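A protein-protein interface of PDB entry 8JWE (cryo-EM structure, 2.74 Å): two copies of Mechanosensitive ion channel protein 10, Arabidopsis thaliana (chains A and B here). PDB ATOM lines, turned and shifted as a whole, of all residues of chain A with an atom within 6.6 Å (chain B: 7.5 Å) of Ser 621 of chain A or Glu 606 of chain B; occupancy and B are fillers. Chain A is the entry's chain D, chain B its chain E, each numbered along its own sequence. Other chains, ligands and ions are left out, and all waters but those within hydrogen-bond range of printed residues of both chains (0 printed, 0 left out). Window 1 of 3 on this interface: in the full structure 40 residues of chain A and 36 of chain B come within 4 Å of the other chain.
The side-chain sulfur of Cys 581 of chain A sits close to the backbone carbonyl oxygen of Ser 621 of chain A, at 3.6 Å.
The side-chain amide nitrogen of Asn 622 of chain A lies within hydrogen-bond range of the backbone carbonyl oxygen of Pro 574 of chain A, at 2.8 Å.
O of Asn 622 of chain A is in hydrogen-bond range of OG of Ser 626 of chain A (2.9 Å).
The backbone NH (N) of Phe 600 of chain B lies within hydrogen-bond range of the backbone carbonyl oxygen (O) of Val 608 of chain B.
O of Arg 580 of chain A sits at hydrogen-bond distance from N of Tyr 623 of chain A.
O of Val 582 of chain A lies within hydrogen-bond range of N of Ser 621 of chain A (3.2 Å).
Among the printed residues, merely in contact across the chains: Pro 574 of chain A with Tyr 609 of chain B (3.9 Å), Pro 619 of chain A with Tyr 609 of chain B (3.5 Å), Ile 620 of chain A with Val 608 of chain B (3.6 Å), Ser 621 of chain A with Lys 607 of chain B (3.3 Å), Ser 621 of chain A with Val 608 of chain B (3.9 Å), Tyr 623 of chain A with Glu 606 of chain B (3.99 Å), Ser 626 of chain A with Asn 605 of chain B (3.8 Å), Ser 626 of chain A with Glu 606 of chain B (3.8 Å), Pro 627 of chain A with Asn 605 of chain B (3.6 Å), Met 629 of chain A with Asn 604 of chain B (3.4 Å) and Met 629 of chain A with Glu 606 of chain B (3.7 Å).
Ser 621 of chain A touches just these residues of chain B: Glu 606 (2.8 Å), Lys 607 (3.3 Å) and Val 608 (3.9 Å).
Of the printed residues of chain A, Glu 606 of chain B touches Ser 621 (2.8 Å), Tyr 623 (3.99 Å), Ser 626 (3.8 Å) and Met 629 (3.7 Å).
Printed residues of chain B within 4 Å of Met 629 of chain A: Asn 604 (3.4 Å) and Glu 606 (3.7 Å).
Of the printed residues of chain B, Tyr 623 of chain A touches Glu 606.
Of the printed residues of chain A, Lys 607 of chain B touches Ser 621, Asn 622 and Ser 626.
The nearest printed residue of chain A that does not touch Glu 606 of chain B is Val 582 of chain A (4.5 Å).
The backbone NH (N) of Asn 622 of chain A sits at hydrogen-bond distance from the backbone carbonyl oxygen (O) of Lys 607 of chain B, 3.1 Å away.
The backbone NH (N) of Lys 607 of chain B lies within hydrogen-bond range of the side-chain hydroxyl (OG) of Ser 626 of chain A (3.2 Å).
The side-chain hydroxyl (OG) of Ser 621 of chain A sits at hydrogen-bond distance from the side-chain carboxylate (OE2) of Glu 606 of chain B (2.8 Å).
The backbone carbonyl oxygen (O) of Asn 604 of chain B lies within hydrogen-bond range of the backbone NH (N) of Gly 630 of chain A (3.0 Å).
The backbone carbonyl oxygen of Ile 620 of chain A sits at hydrogen-bond distance from the backbone NH of Tyr 609 of chain B (2.9 Å).
No position is printed for both chains.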
ATOM      1  N   PRO A 574     -13.445 -10.463   6.699  1.00  0.00           N
ATOM      2  CA  PRO A 574     -13.737  -9.074   6.945  1.00  0.00           C
ATOM      3  C   PRO A 574     -14.566  -8.770   8.150  1.00  0.00           C
ATOM      4  O   PRO A 574     -14.724  -7.607   8.424  1.00  0.00           O
ATOM      5  CB  PRO A 574     -14.442  -8.691   5.686  1.00  0.00           C
ATOM      6  CG  PRO A 574     -14.950  -9.737   5.247  1.00  0.00           C
ATOM      7  CD  PRO A 574     -14.199 -10.865   5.524  1.00  0.00           C
ATOM      8  N   TYR A 575     -15.092  -9.739   8.881  1.00  0.00           N
ATOM      9  CA  TYR A 575     -15.943  -9.539  10.042  1.00  0.00           C
ATOM     10  C   TYR A 575     -15.909 -10.776  10.906  1.00  0.00           C
ATOM     11  O   TYR A 575     -15.438 -11.803  10.492  1.00  0.00           O
ATOM     12  CB  TYR A 575     -17.391  -9.191   9.683  1.00  0.00           C
ATOM     13  CG  TYR A 575     -18.043  -9.968   8.611  1.00  0.00           C
ATOM     14  CD1 TYR A 575     -18.246  -9.416   7.423  1.00  0.00           C
ATOM     15  CD2 TYR A 575     -18.423 -11.252   8.783  1.00  0.00           C
ATOM     16  CE1 TYR A 575     -18.789 -10.075   6.486  1.00  0.00           C
ATOM     17  CE2 TYR A 575     -18.932 -11.922   7.811  1.00  0.00           C
ATOM     18  CZ  TYR A 575     -19.127 -11.324   6.690  1.00  0.00           C
ATOM     19  OH  TYR A 575     -19.646 -11.986   5.715  1.00  0.00           O
ATOM     20  N   ARG A 580     -21.425  -4.954  13.181  1.00  0.00           N
ATOM     21  CA  ARG A 580     -22.331  -4.296  12.288  1.00  0.00           C
ATOM     22  C   ARG A 580     -21.545  -3.829  11.096  1.00  0.00           C
ATOM     23  O   ARG A 580     -20.499  -3.258  11.239  1.00  0.00           O
ATOM     24  CB  ARG A 580     -23.043  -3.163  12.993  1.00  0.00           C
ATOM     25  CG  ARG A 580     -24.283  -2.830  12.358  1.00  0.00           C
ATOM     26  CD  ARG A 580     -24.969  -1.729  12.899  1.00  0.00           C
ATOM     27  NE  ARG A 580     -25.292  -1.795  14.310  1.00  0.00           N
ATOM     28  CZ  ARG A 580     -26.333  -2.377  14.849  1.00  0.00           C
ATOM     29  NH1 ARG A 580     -27.182  -3.016  14.144  1.00  0.00           N
ATOM     30  NH2 ARG A 580     -26.496  -2.326  16.105  1.00  0.00           N
ATOM     31  N   CYS A 581     -22.022  -4.141   9.935  1.00  0.00           N
ATOM     32  CA  CYS A 581     -21.301  -4.113   8.701  1.00  0.00           C
ATOM     33  C   CYS A 581     -22.165  -3.395   7.693  1.00  0.00           C
ATOM     34  O   CYS A 581     -23.294  -3.138   7.971  1.00  0.00           O
ATOM     35  CB  CYS A 581     -20.950  -5.523   8.279  1.00  0.00           C
ATOM     36  SG  CYS A 581     -19.751  -6.205   9.233  1.00  0.00           S
ATOM     37  N   VAL A 582     -21.650  -2.969   6.566  1.00  0.00           N
ATOM     38  CA  VAL A 582     -22.441  -2.310   5.540  1.00  0.00           C
ATOM     39  C   VAL A 582     -22.152  -3.001   4.232  1.00  0.00           C
ATOM     40  O   VAL A 582     -21.002  -3.176   3.888  1.00  0.00           O
ATOM     41  CB  VAL A 582     -22.120  -0.812   5.419  1.00  0.00           C
ATOM     42  CG1 VAL A 582     -22.943  -0.216   4.501  1.00  0.00           C
ATOM     43  CG2 VAL A 582     -22.376  -0.150   6.564  1.00  0.00           C
ATOM     44  N   VAL A 583     -23.158  -3.424   3.506  1.00  0.00           N
ATOM     45  CA  VAL A 583     -22.929  -4.239   2.333  1.00  0.00           C
ATOM     46  C   VAL A 583     -23.310  -3.536   1.051  1.00  0.00           C
ATOM     47  O   VAL A 583     -22.509  -3.475   0.125  1.00  0.00           O
ATOM     48  CB  VAL A 583     -23.577  -5.624   2.441  1.00  0.00           C
ATOM     49  CG1 VAL A 583     -23.345  -6.340   1.231  1.00  0.00           C
ATOM     50  CG2 VAL A 583     -22.888  -6.386   3.489  1.00  0.00           C
ATOM     51  N   PRO A 619     -17.145  -4.501  -1.809  1.00  0.00           N
ATOM     52  CA  PRO A 619     -16.587  -3.827  -0.635  1.00  0.00           C
ATOM     53  C   PRO A 619     -17.470  -3.894   0.607  1.00  0.00           C
ATOM     54  O   PRO A 619     -18.658  -3.614   0.543  1.00  0.00           O
ATOM     55  CB  PRO A 619     -16.450  -2.405  -1.128  1.00  0.00           C
ATOM     56  CG  PRO A 619     -17.238  -2.305  -2.122  1.00  0.00           C
ATOM     57  CD  PRO A 619     -17.366  -3.521  -2.847  1.00  0.00           C
ATOM     58  N   ILE A 620     -16.890  -4.235   1.743  1.00  0.00           N
ATOM     59  CA  ILE A 620     -17.623  -4.468   2.978  1.00  0.00           C
ATOM     60  C   ILE A 620     -17.077  -3.565   4.049  1.00  0.00           C
ATOM     61  O   ILE A 620     -15.892  -3.551   4.264  1.00  0.00           O
ATOM     62  CB  ILE A 620     -17.546  -5.949   3.391  1.00  0.00           C
ATOM     63  CG1 ILE A 620     -18.232  -6.787   2.365  1.00  0.00           C
ATOM     64  CG2 ILE A 620     -18.248  -6.199   4.626  1.00  0.00           C
ATOM     65  CD1 ILE A 620     -17.951  -8.052   2.390  1.00  0.00           C
ATOM     66  N   SER A 621     -17.920  -2.820   4.721  1.00  0.00           N
ATOM     67  CA  SER A 621     -17.512  -1.963   5.809  1.00  0.00           C
ATOM     68  C   SER A 621     -17.696  -2.652   7.128  1.00  0.00           C
ATOM     69  O   SER A 621     -18.542  -3.474   7.262  1.00  0.00           O
ATOM     70  CB  SER A 621     -18.313  -0.706   5.834  1.00  0.00           C
ATOM     71  OG  SER A 621     -18.365  -0.100   4.606  1.00  0.00           O
ATOM     72  N   ASN A 622     -16.940  -2.286   8.120  1.00  0.00           N
ATOM     73  CA  ASN A 622     -17.053  -2.904   9.418  1.00  0.00           C
ATOM     74  C   ASN A 622     -16.999  -1.788  10.434  1.00  0.00           C
ATOM     75  O   ASN A 622     -15.998  -1.118  10.538  1.00  0.00           O
ATOM     76  CB  ASN A 622     -15.944  -3.921   9.582  1.00  0.00           C
ATOM     77  CG  ASN A 622     -16.111  -4.841  10.693  1.00  0.00           C
ATOM     78  OD1 ASN A 622     -16.752  -4.611  11.612  1.00  0.00           O
ATOM     79  ND2 ASN A 622     -15.594  -5.934  10.534  1.00  0.00           N
ATOM     80  N   TYR A 623     -18.072  -1.558  11.144  1.00  0.00           N
ATOM     81  CA  TYR A 623     -18.134  -0.477  12.103  1.00  0.00           C
ATOM     82  C   TYR A 623     -17.466  -0.794  13.390  1.00  0.00           C
ATOM     83  O   TYR A 623     -17.080   0.103  14.078  1.00  0.00           O
ATOM     84  CB  TYR A 623     -19.544  -0.114  12.438  1.00  0.00           C
ATOM     85  CG  TYR A 623     -20.327   0.604  11.440  1.00  0.00           C
ATOM     86  CD1 TYR A 623     -19.755   1.415  10.532  1.00  0.00           C
ATOM     87  CD2 TYR A 623     -21.652   0.409  11.378  1.00  0.00           C
ATOM     88  CE1 TYR A 623     -20.497   2.033   9.645  1.00  0.00           C
ATOM     89  CE2 TYR A 623     -22.369   0.991  10.526  1.00  0.00           C
ATOM     90  CZ  TYR A 623     -21.811   1.807   9.657  1.00  0.00           C
ATOM     91  OH  TYR A 623     -22.614   2.395   8.772  1.00  0.00           O
ATOM     92  N   SER A 626     -13.519  -0.027  13.237  1.00  0.00           N
ATOM     93  CA  SER A 626     -13.281   1.348  12.865  1.00  0.00           C
ATOM     94  C   SER A 626     -12.787   2.196  14.023  1.00  0.00           C
ATOM     95  O   SER A 626     -12.994   1.860  15.164  1.00  0.00           O
ATOM     96  CB  SER A 626     -14.541   1.964  12.346  1.00  0.00           C
ATOM     97  OG  SER A 626     -14.889   1.447  11.154  1.00  0.00           O
ATOM     98  N   PRO A 627     -12.114   3.308  13.739  1.00  0.00           N
ATOM     99  CA  PRO A 627     -11.930   4.359  14.734  1.00  0.00           C
ATOM    100  C   PRO A 627     -13.236   5.069  15.036  1.00  0.00           C
ATOM    101  O   PRO A 627     -14.227   4.848  14.381  1.00  0.00           O
ATOM    102  CB  PRO A 627     -10.983   5.284  14.014  1.00  0.00           C
ATOM    103  CG  PRO A 627     -10.486   4.586  13.029  1.00  0.00           C
ATOM    104  CD  PRO A 627     -11.302   3.587  12.570  1.00  0.00           C
ATOM    105  N   MET A 629     -16.128   7.630  14.861  1.00  0.00           N
ATOM    106  CA  MET A 629     -16.647   8.021  13.572  1.00  0.00           C
ATOM    107  C   MET A 629     -17.215   9.420  13.579  1.00  0.00           C
ATOM    108  O   MET A 629     -17.474   9.980  14.609  1.00  0.00           O
ATOM    109  CB  MET A 629     -17.663   6.988  13.132  1.00  0.00           C
ATOM    110  CG  MET A 629     -17.052   5.746  12.607  1.00  0.00           C
ATOM    111  SD  MET A 629     -17.988   4.368  12.172  1.00  0.00           S
ATOM    112  CE  MET A 629     -18.625   5.075  10.803  1.00  0.00           C
ATOM    113  N   GLY A 630     -17.404  10.000  12.408  1.00  0.00           N
ATOM    114  CA  GLY A 630     -17.822  11.383  12.277  1.00  0.00           C
ATOM    115  C   GLY A 630     -19.254  11.670  11.872  1.00  0.00           C
ATOM    116  O   GLY A 630     -19.836  10.929  11.152  1.00  0.00           O
ATOM    117  N   PHE A 693     -20.376   3.614  14.720  1.00  0.00           N
ATOM    118  CA  PHE A 693     -21.779   3.447  14.409  1.00  0.00           C
ATOM    119  C   PHE A 693     -22.266   2.065  14.687  1.00  0.00           C
ATOM    120  O   PHE A 693     -23.325   1.752  14.238  1.00  0.00           O
ATOM    121  CB  PHE A 693     -22.110   3.766  12.967  1.00  0.00           C
ATOM    122  CG  PHE A 693     -21.997   5.174  12.580  1.00  0.00           C
ATOM    123  CD1 PHE A 693     -21.733   6.177  13.463  1.00  0.00           C
ATOM    124  CD2 PHE A 693     -22.167   5.510  11.300  1.00  0.00           C
ATOM    125  CE1 PHE A 693     -21.588   7.412  13.063  1.00  0.00           C
ATOM    126  CE2 PHE A 693     -22.043   6.780  10.918  1.00  0.00           C
ATOM    127  CZ  PHE A 693     -21.765   7.714  11.818  1.00  0.00           C
ATOM    128  N   MET B 588     -10.931   7.865  -0.113  1.00  0.00           N
ATOM    129  CA  MET B 588     -10.597   6.806   0.821  1.00  0.00           C
ATOM    130  C   MET B 588      -9.116   6.745   1.109  1.00  0.00           C
ATOM    131  O   MET B 588      -8.350   6.509   0.215  1.00  0.00           O
ATOM    132  CB  MET B 588     -11.009   5.495   0.226  1.00  0.00           C
ATOM    133  CG  MET B 588     -12.382   5.031   0.328  1.00  0.00           C
ATOM    134  SD  MET B 588     -12.436   3.800  -0.907  1.00  0.00           S
ATOM    135  CE  MET B 588     -13.755   2.953  -0.328  1.00  0.00           C
ATOM    136  N   LEU B 589      -8.723   6.789   2.342  1.00  0.00           N
ATOM    137  CA  LEU B 589      -7.336   6.690   2.729  1.00  0.00           C
ATOM    138  C   LEU B 589      -6.865   5.261   2.863  1.00  0.00           C
ATOM    139  O   LEU B 589      -7.528   4.474   3.477  1.00  0.00           O
ATOM    140  CB  LEU B 589      -7.194   7.383   4.039  1.00  0.00           C
ATOM    141  CG  LEU B 589      -5.935   7.747   4.669  1.00  0.00           C
ATOM    142  CD1 LEU B 589      -5.472   8.805   3.992  1.00  0.00           C
ATOM    143  CD2 LEU B 589      -6.359   8.227   5.889  1.00  0.00           C
ATOM    144  N   GLU B 591      -4.845   2.250   4.404  1.00  0.00           N
ATOM    145  CA  GLU B 591      -3.959   1.905   5.485  1.00  0.00           C
ATOM    146  C   GLU B 591      -3.501   0.489   5.611  1.00  0.00           C
ATOM    147  O   GLU B 591      -2.665   0.240   6.458  1.00  0.00           O
ATOM    148  CB  GLU B 591      -4.530   2.283   6.825  1.00  0.00           C
ATOM    149  CG  GLU B 591      -5.424   1.411   7.344  1.00  0.00           C
ATOM    150  CD  GLU B 591      -6.678   1.745   7.029  1.00  0.00           C
ATOM    151  OE1 GLU B 591      -6.879   2.731   6.395  1.00  0.00           O
ATOM    152  OE2 GLU B 591      -7.517   0.960   7.369  1.00  0.00           O
ATOM    153  N   PHE B 600      -9.274   0.445   3.609  1.00  0.00           N
ATOM    154  CA  PHE B 600      -9.423   1.871   3.419  1.00  0.00           C
ATOM    155  C   PHE B 600     -10.086   2.518   4.622  1.00  0.00           C
ATOM    156  O   PHE B 600     -10.691   1.868   5.408  1.00  0.00           O
ATOM    157  CB  PHE B 600     -10.238   2.151   2.185  1.00  0.00           C
ATOM    158  CG  PHE B 600      -9.595   1.822   0.906  1.00  0.00           C
ATOM    159  CD1 PHE B 600      -8.711   2.649   0.350  1.00  0.00           C
ATOM    160  CD2 PHE B 600      -9.979   0.742   0.186  1.00  0.00           C
ATOM    161  CE1 PHE B 600      -8.193   2.392  -0.831  1.00  0.00           C
ATOM    162  CE2 PHE B 600      -9.431   0.501  -1.012  1.00  0.00           C
ATOM    163  CZ  PHE B 600      -8.547   1.329  -1.501  1.00  0.00           C
ATOM    164  N   LEU B 601      -9.973   3.805   4.804  1.00  0.00           N
ATOM    165  CA  LEU B 601     -10.848   4.548   5.701  1.00  0.00           C
ATOM    166  C   LEU B 601     -11.556   5.631   4.941  1.00  0.00           C
ATOM    167  O   LEU B 601     -10.946   6.313   4.158  1.00  0.00           O
ATOM    168  CB  LEU B 601     -10.152   5.224   6.832  1.00  0.00           C
ATOM    169  CG  LEU B 601      -9.408   4.484   7.884  1.00  0.00           C
ATOM    170  CD1 LEU B 601      -8.943   5.460   8.742  1.00  0.00           C
ATOM    171  CD2 LEU B 601     -10.216   3.574   8.604  1.00  0.00           C
ATOM    172  N   LYS B 602     -12.818   5.818   5.178  1.00  0.00           N
ATOM    173  CA  LYS B 602     -13.552   6.865   4.522  1.00  0.00           C
ATOM    174  C   LYS B 602     -13.421   8.196   5.216  1.00  0.00           C
ATOM    175  O   LYS B 602     -12.729   8.339   6.197  1.00  0.00           O
ATOM    176  CB  LYS B 602     -14.977   6.503   4.462  1.00  0.00           C
ATOM    177  CG  LYS B 602     -15.190   5.521   3.599  1.00  0.00           C
ATOM    178  CD  LYS B 602     -16.505   5.438   3.557  1.00  0.00           C
ATOM    179  CE  LYS B 602     -16.802   4.571   2.590  1.00  0.00           C
ATOM    180  NZ  LYS B 602     -18.187   4.703   2.500  1.00  0.00           N
ATOM    181  N   LEU B 603     -14.091   9.199   4.708  1.00  0.00           N
ATOM    182  CA  LEU B 603     -13.967  10.502   5.323  1.00  0.00           C
ATOM    183  C   LEU B 603     -14.669  10.619   6.662  1.00  0.00           C
ATOM    184  O   LEU B 603     -14.297  11.488   7.422  1.00  0.00           O
ATOM    185  CB  LEU B 603     -14.457  11.596   4.400  1.00  0.00           C
ATOM    186  CG  LEU B 603     -13.695  12.021   3.154  1.00  0.00           C
ATOM    187  CD1 LEU B 603     -14.441  12.925   2.372  1.00  0.00           C
ATOM    188  CD2 LEU B 603     -12.441  12.636   3.498  1.00  0.00           C
ATOM    189  N   ASN B 604     -15.601   9.738   6.998  1.00  0.00           N
ATOM    190  CA  ASN B 604     -16.172   9.629   8.318  1.00  0.00           C
ATOM    191  C   ASN B 604     -15.485   8.632   9.225  1.00  0.00           C
ATOM    192  O   ASN B 604     -15.944   8.463  10.319  1.00  0.00           O
ATOM    193  CB  ASN B 604     -17.649   9.296   8.258  1.00  0.00           C
ATOM    194  CG  ASN B 604     -17.973   8.016   7.600  1.00  0.00           C
ATOM    195  OD1 ASN B 604     -17.174   7.375   7.016  1.00  0.00           O
ATOM    196  ND2 ASN B 604     -19.173   7.618   7.739  1.00  0.00           N
ATOM    197  N   ASN B 605     -14.373   8.047   8.811  1.00  0.00           N
ATOM    198  CA  ASN B 605     -13.525   7.043   9.427  1.00  0.00           C
ATOM    199  C   ASN B 605     -14.093   5.660   9.422  1.00  0.00           C
ATOM    200  O   ASN B 605     -13.659   4.887  10.145  1.00  0.00           O
ATOM    201  CB  ASN B 605     -13.123   7.265  10.877  1.00  0.00           C
ATOM    202  CG  ASN B 605     -12.458   8.478  11.106  1.00  0.00           C
ATOM    203  OD1 ASN B 605     -12.821   9.211  11.962  1.00  0.00           O
ATOM    204  ND2 ASN B 605     -11.489   8.742  10.358  1.00  0.00           N
ATOM    205  N   GLU B 606     -15.054   5.356   8.621  1.00  0.00           N
ATOM    206  CA  GLU B 606     -15.510   4.007   8.435  1.00  0.00           C
ATOM    207  C   GLU B 606     -14.522   3.182   7.625  1.00  0.00           C
ATOM    208  O   GLU B 606     -13.996   3.634   6.637  1.00  0.00           O
ATOM    209  CB  GLU B 606     -16.835   4.107   7.764  1.00  0.00           C
ATOM    210  CG  GLU B 606     -17.387   2.970   7.229  1.00  0.00           C
ATOM    211  CD  GLU B 606     -18.553   3.282   6.388  1.00  0.00           C
ATOM    212  OE1 GLU B 606     -19.103   4.339   6.455  1.00  0.00           O
ATOM    213  OE2 GLU B 606     -18.897   2.512   5.523  1.00  0.00           O
ATOM    214  N   LYS B 607     -14.285   1.956   8.051  1.00  0.00           N
ATOM    215  CA  LYS B 607     -13.262   1.086   7.521  1.00  0.00           C
ATOM    216  C   LYS B 607     -13.806   0.095   6.520  1.00  0.00           C
ATOM    217  O   LYS B 607     -14.724  -0.608   6.821  1.00  0.00           O
ATOM    218  CB  LYS B 607     -12.613   0.376   8.678  1.00  0.00           C
ATOM    219  CG  LYS B 607     -11.719  -0.631   8.314  1.00  0.00           C
ATOM    220  CD  LYS B 607     -11.029  -1.177   9.400  1.00  0.00           C
ATOM    221  CE  LYS B 607      -9.927  -0.364   9.752  1.00  0.00           C
ATOM    222  NZ  LYS B 607      -9.118  -0.967  10.719  1.00  0.00           N
ATOM    223  N   VAL B 608     -13.225   0.028   5.346  1.00  0.00           N
ATOM    224  CA  VAL B 608     -13.744  -0.707   4.209  1.00  0.00           C
ATOM    225  C   VAL B 608     -12.718  -1.747   3.820  1.00  0.00           C
ATOM    226  O   VAL B 608     -11.539  -1.463   3.786  1.00  0.00           O
ATOM    227  CB  VAL B 608     -14.039   0.224   3.015  1.00  0.00           C
ATOM    228  CG1 VAL B 608     -14.627  -0.463   1.925  1.00  0.00           C
ATOM    229  CG2 VAL B 608     -14.895   1.241   3.357  1.00  0.00           C
ATOM    230  N   TYR B 609     -13.162  -2.942   3.515  1.00  0.00           N
ATOM    231  CA  TYR B 609     -12.356  -4.031   3.018  1.00  0.00           C
ATOM    232  C   TYR B 609     -12.687  -4.257   1.563  1.00  0.00           C
ATOM    233  O   TYR B 609     -13.746  -4.743   1.263  1.00  0.00           O
ATOM    234  CB  TYR B 609     -12.641  -5.284   3.822  1.00  0.00           C
ATOM    235  CG  TYR B 609     -12.165  -5.261   5.213  1.00  0.00           C
ATOM    236  CD1 TYR B 609     -10.989  -5.783   5.531  1.00  0.00           C
ATOM    237  CD2 TYR B 609     -12.886  -4.667   6.204  1.00  0.00           C
ATOM    238  CE1 TYR B 609     -10.561  -5.736   6.722  1.00  0.00           C
ATOM    239  CE2 TYR B 609     -12.432  -4.601   7.381  1.00  0.00           C
ATOM    240  CZ  TYR B 609     -11.276  -5.156   7.623  1.00  0.00           C
ATOM    241  OH  TYR B 609     -10.764  -5.138   8.813  1.00  0.00           O
ATOM    242  N   TYR B 610     -11.765  -3.990   0.665  1.00  0.00           N
ATOM    243  CA  TYR B 610     -12.049  -3.998  -0.758  1.00  0.00           C
ATOM    244  C   TYR B 610     -11.223  -5.069  -1.423  1.00  0.00           C
ATOM    245  O   TYR B 610     -10.016  -5.010  -1.321  1.00  0.00           O
ATOM    246  CB  TYR B 610     -11.681  -2.672  -1.360  1.00  0.00           C
ATOM    247  CG  TYR B 610     -11.813  -2.517  -2.807  1.00  0.00           C
ATOM    248  CD1 TYR B 610     -13.018  -2.336  -3.366  1.00  0.00           C
ATOM    249  CD2 TYR B 610     -10.749  -2.688  -3.625  1.00  0.00           C
ATOM    250  CE1 TYR B 610     -13.146  -2.212  -4.624  1.00  0.00           C
ATOM    251  CE2 TYR B 610     -10.875  -2.601  -4.910  1.00  0.00           C
ATOM    252  CZ  TYR B 610     -12.077  -2.360  -5.396  1.00  0.00           C
ATOM    253  OH  TYR B 610     -12.198  -2.273  -6.707  1.00  0.00           O
